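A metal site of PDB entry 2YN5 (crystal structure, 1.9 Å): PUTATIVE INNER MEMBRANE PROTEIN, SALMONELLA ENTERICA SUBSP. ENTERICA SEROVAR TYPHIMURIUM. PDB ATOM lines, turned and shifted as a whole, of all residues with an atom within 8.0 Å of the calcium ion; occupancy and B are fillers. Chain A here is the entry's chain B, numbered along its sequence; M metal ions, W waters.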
ATOM      1  N   LEU A  90     -33.269 -24.548  30.375  1.00  0.00           N
ATOM      2  CA  LEU A  90     -31.888 -24.845  30.677  1.00  0.00           C
ATOM      3  C   LEU A  90     -31.153 -23.555  31.121  1.00  0.00           C
ATOM      4  O   LEU A  90     -31.185 -22.544  30.419  1.00  0.00           O
ATOM      5  CB  LEU A  90     -31.225 -25.427  29.430  1.00  0.00           C
ATOM      6  CG  LEU A  90     -29.741 -25.824  29.454  1.00  0.00           C
ATOM      7  CD1 LEU A  90     -29.465 -26.980  30.412  1.00  0.00           C
ATOM      8  CD2 LEU A  90     -29.333 -26.199  28.044  1.00  0.00           C
ATOM      9  N   PRO A  92     -28.443 -20.780  31.418  1.00  0.00           N
ATOM     10  CA  PRO A  92     -27.338 -20.428  30.506  1.00  0.00           C
ATOM     11  C   PRO A  92     -25.978 -20.912  30.992  1.00  0.00           C
ATOM     12  O   PRO A  92     -25.132 -21.238  30.181  1.00  0.00           O
ATOM     13  CB  PRO A  92     -27.378 -18.886  30.443  1.00  0.00           C
ATOM     14  CG  PRO A  92     -28.711 -18.489  30.975  1.00  0.00           C
ATOM     15  CD  PRO A  92     -29.282 -19.627  31.794  1.00  0.00           C
ATOM     16  N   SER A  94     -25.459 -23.772  32.333  1.00  0.00           N
ATOM     17  CA  SER A  94     -25.384 -25.192  32.013  1.00  0.00           C
ATOM     18  C   SER A  94     -25.537 -25.459  30.523  1.00  0.00           C
ATOM     19  O   SER A  94     -25.814 -26.580  30.120  1.00  0.00           O
ATOM     20  CB  SER A  94     -26.513 -25.927  32.740  1.00  0.00           C
ATOM     21  OG  SER A  94     -26.303 -25.901  34.129  1.00  0.00           O
ATOM     22  N   ASP A  95     -25.425 -24.425  29.705  1.00  0.00           N
ATOM     23  CA  ASP A  95     -25.677 -24.533  28.253  1.00  0.00           C
ATOM     24  C   ASP A  95     -24.355 -24.356  27.512  1.00  0.00           C
ATOM     25  O   ASP A  95     -23.942 -23.225  27.205  1.00  0.00           O
ATOM     26  CB  ASP A  95     -26.725 -23.477  27.827  1.00  0.00           C
ATOM     27  CG  ASP A  95     -27.083 -23.525  26.327  1.00  0.00           C
ATOM     28  OD1 ASP A  95     -26.730 -24.468  25.587  1.00  0.00           O
ATOM     29  OD2 ASP A  95     -27.768 -22.572  25.872  1.00  0.00           O
ATOM     30  N   SER A  96     -23.660 -25.455  27.259  1.00  0.00           N
ATOM     31  CA  SER A  96     -22.323 -25.365  26.680  1.00  0.00           C
ATOM     32  C   SER A  96     -22.331 -25.184  25.175  1.00  0.00           C
ATOM     33  O   SER A  96     -23.359 -25.372  24.502  1.00  0.00           O
ATOM     34  CB  SER A  96     -21.503 -26.598  27.047  1.00  0.00           C
ATOM     35  OG  SER A  96     -21.949 -27.702  26.287  1.00  0.00           O
ATOM     36  N   GLY A  97     -21.155 -24.846  24.643  1.00  0.00           N
ATOM     37  CA  GLY A  97     -20.970 -24.678  23.219  1.00  0.00           C
ATOM     38  C   GLY A  97     -21.861 -23.530  22.797  1.00  0.00           C
ATOM     39  O   GLY A  97     -21.946 -22.537  23.496  1.00  0.00           O
ATOM     40  N   THR A  98     -22.514 -23.670  21.650  1.00  0.00           N
ATOM     41  CA  THR A  98     -23.523 -22.710  21.159  1.00  0.00           C
ATOM     42  C   THR A  98     -24.583 -22.452  22.214  1.00  0.00           C
ATOM     43  O   THR A  98     -25.221 -23.372  22.711  1.00  0.00           O
ATOM     44  CB  THR A  98     -24.214 -23.284  19.904  1.00  0.00           C
ATOM     45  OG1 THR A  98     -23.214 -23.686  18.962  1.00  0.00           O
ATOM     46  CG2 THR A  98     -25.212 -22.297  19.279  1.00  0.00           C
ATOM     47  N   VAL A  99     -24.819 -21.197  22.543  1.00  0.00           N
ATOM     48  CA  VAL A  99     -25.811 -20.866  23.562  1.00  0.00           C
ATOM     49  C   VAL A  99     -27.180 -20.777  22.870  1.00  0.00           C
ATOM     50  O   VAL A  99     -27.293 -20.234  21.771  1.00  0.00           O
ATOM     51  CB  VAL A  99     -25.474 -19.570  24.333  1.00  0.00           C
ATOM     52  CG1 VAL A  99     -26.281 -19.490  25.616  1.00  0.00           C
ATOM     53  CG2 VAL A  99     -23.987 -19.502  24.670  1.00  0.00           C
ATOM     54  N   GLY A 100     -28.201 -21.343  23.503  1.00  0.00           N
ATOM     55  CA  GLY A 100     -29.587 -21.148  23.052  1.00  0.00           C
ATOM     56  C   GLY A 100     -30.222 -22.354  22.408  1.00  0.00           C
ATOM     57  O   GLY A 100     -31.437 -22.347  22.129  1.00  0.00           O
ATOM     58  N   ASP A 101     -29.430 -23.402  22.182  1.00  0.00           N
ATOM     59  CA  ASP A 101     -29.878 -24.519  21.358  1.00  0.00           C
ATOM     60  C   ASP A 101     -30.368 -25.736  22.148  1.00  0.00           C
ATOM     61  O   ASP A 101     -30.721 -26.732  21.556  1.00  0.00           O
ATOM     62  CB  ASP A 101     -28.780 -24.910  20.358  1.00  0.00           C
ATOM     63  CG  ASP A 101     -27.518 -25.454  21.029  1.00  0.00           C
ATOM     64  OD1 ASP A 101     -27.418 -25.469  22.279  1.00  0.00           O
ATOM     65  OD2 ASP A 101     -26.607 -25.870  20.309  1.00  0.00           O
ATOM     66  N   ASN A 102     -30.369 -25.654  23.485  1.00  0.00           N
ATOM     67  CA  ASN A 102     -30.778 -26.795  24.315  1.00  0.00           C
ATOM     68  C   ASN A 102     -29.949 -28.067  24.115  1.00  0.00           C
ATOM     69  O   ASN A 102     -30.439 -29.188  24.318  1.00  0.00           O
ATOM     70  CB  ASN A 102     -32.278 -27.083  24.132  1.00  0.00           C
ATOM     71  CG  ASN A 102     -33.124 -26.177  24.975  1.00  0.00           C
ATOM     72  OD1 ASN A 102     -32.623 -25.580  25.908  1.00  0.00           O
ATOM     73  ND2 ASN A 102     -34.383 -26.031  24.633  1.00  0.00           N
ATOM     74  N   ILE A 103     -28.695 -27.882  23.694  1.00  0.00           N
ATOM     75  CA  ILE A 103     -27.743 -28.995  23.613  1.00  0.00           C
ATOM     76  C   ILE A 103     -26.627 -28.629  24.561  1.00  0.00           C
ATOM     77  O   ILE A 103     -26.158 -27.516  24.514  1.00  0.00           O
ATOM     78  CB  ILE A 103     -27.159 -29.166  22.207  1.00  0.00           C
ATOM     79  CG1 ILE A 103     -28.265 -29.348  21.154  1.00  0.00           C
ATOM     80  CG2 ILE A 103     -26.140 -30.333  22.208  1.00  0.00           C
ATOM     81  CD1 ILE A 103     -27.747 -29.297  19.714  1.00  0.00           C
ATOM     82  N   THR A 104     -26.171 -29.560  25.388  1.00  0.00           N
ATOM     83  CA  THR A 104     -25.108 -29.203  26.316  1.00  0.00           C
ATOM     84  C   THR A 104     -24.288 -30.423  26.661  1.00  0.00           C
ATOM     85  O   THR A 104     -24.810 -31.520  26.603  1.00  0.00           O
ATOM     86  CB  THR A 104     -25.694 -28.606  27.597  1.00  0.00           C
ATOM     87  OG1 THR A 104     -24.624 -28.216  28.468  1.00  0.00           O
ATOM     88  CG2 THR A 104     -26.607 -29.634  28.318  1.00  0.00           C
ATOM     89  N   ARG A 105     -23.023 -30.237  27.025  1.00  0.00           N
ATOM     90  CA  ARG A 105     -22.232 -31.353  27.534  1.00  0.00           C
ATOM     91  C   ARG A 105     -22.332 -31.499  29.049  1.00  0.00           C
ATOM     92  O   ARG A 105     -21.710 -32.387  29.626  1.00  0.00           O
ATOM     93  CB  ARG A 105     -20.755 -31.274  27.051  1.00  0.00           C
ATOM     94  CG  ARG A 105     -19.919 -30.155  27.662  1.00  0.00           C
ATOM     95  CD  ARG A 105     -18.464 -30.237  27.193  1.00  0.00           C
ATOM     96  NE  ARG A 105     -17.572 -29.381  27.978  1.00  0.00           N
ATOM     97  CZ  ARG A 105     -17.394 -28.071  27.761  1.00  0.00           C
ATOM     98  NH1 ARG A 105     -18.038 -27.454  26.752  1.00  0.00           N
ATOM     99  NH2 ARG A 105     -16.560 -27.386  28.540  1.00  0.00           N
ATOM    100  N   THR A 177     -30.745 -32.016  24.834  1.00  0.00           N
ATOM    101  CA  THR A 177     -29.819 -33.049  24.379  1.00  0.00           C
ATOM    102  C   THR A 177     -28.563 -32.966  25.202  1.00  0.00           C
ATOM    103  O   THR A 177     -27.882 -31.909  25.236  1.00  0.00           O
ATOM    104  CB  THR A 177     -29.522 -32.909  22.874  1.00  0.00           C
ATOM    105  OG1 THR A 177     -30.743 -33.018  22.163  1.00  0.00           O
ATOM    106  CG2 THR A 177     -28.602 -34.026  22.383  1.00  0.00           C
ATOM    107  N   ARG A 267     -20.783 -29.340  18.496  1.00  0.00           N
ATOM    108  CA  ARG A 267     -21.738 -28.285  18.903  1.00  0.00           C
ATOM    109  C   ARG A 267     -21.792 -28.016  20.405  1.00  0.00           C
ATOM    110  O   ARG A 267     -22.034 -26.872  20.825  1.00  0.00           O
ATOM    111  CB  ARG A 267     -23.133 -28.650  18.442  1.00  0.00           C
ATOM    112  CG  ARG A 267     -23.287 -28.851  16.966  1.00  0.00           C
ATOM    113  CD  ARG A 267     -24.733 -29.249  16.696  1.00  0.00           C
ATOM    114  NE  ARG A 267     -25.046 -30.588  17.206  1.00  0.00           N
ATOM    115  CZ  ARG A 267     -26.210 -31.190  16.979  1.00  0.00           C
ATOM    116  NH1 ARG A 267     -27.170 -30.557  16.295  1.00  0.00           N
ATOM    117  NH2 ARG A 267     -26.441 -32.416  17.466  1.00  0.00           N
ATOM    118  N   ALA A 268     -21.563 -29.058  21.215  1.00  0.00           N
ATOM    119  CA  ALA A 268     -21.629 -28.935  22.660  1.00  0.00           C
ATOM    120  C   ALA A 268     -20.318 -28.410  23.265  1.00  0.00           C
ATOM    121  O   ALA A 268     -20.210 -28.213  24.487  1.00  0.00           O
ATOM    122  CB  ALA A 268     -21.994 -30.295  23.255  1.00  0.00           C
ATOM    123  N   GLY A 269     -19.326 -28.198  22.411  1.00  0.00           N
ATOM    124  CA  GLY A 269     -18.030 -27.675  22.840  1.00  0.00           C
ATOM    125  C   GLY A 269     -17.127 -28.754  23.354  1.00  0.00           C
ATOM    126  O   GLY A 269     -16.070 -28.448  23.920  1.00  0.00           O
HETATM  127 CA    CA M   1     -25.519 -25.425  23.796  1.00  0.00          CA
HETATM  128  O   HOH W   1     -24.625 -26.643  21.863  1.00  0.00           O
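The calcium ion is bound by O of Ser 96 (2.3 Å), O of Ile 103 (2.3 Å), O of Thr 98 (2.3 Å), OD1 of Asp 95 (2.4 Å), OD1 of Asp 101 (2.4 Å) and water W1 (2.5 Å). The calcium ion has six donor atoms within binding distance.
The backbone carbonyl oxygen (O) of Arg 267 lies within hydrogen-bond range of the backbone NH (N) of Thr 98. OG1 of Thr 104 lies within hydrogen-bond range of N of Ser 96 (3.2 Å). OD2 of Asp 95 is in hydrogen-bond range of N of Gly 100, 2.7 Å away. The backbone NH (N) of Arg 105 lies within hydrogen-bond range of the side-chain hydroxyl (OG) of Ser 96, at 2.9 Å. O of Ala 268 is in hydrogen-bond range of OG of Ser 96, at 2.6 Å.
Within 4 Å of the calcium ion: Asp 95, Ser 96, Thr 98, Asp 101 and Ile 103.
Water W1 lies within hydrogen-bond range of OD2 of Asp 101 (2.6 Å) and O of Arg 267 (2.8 Å).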
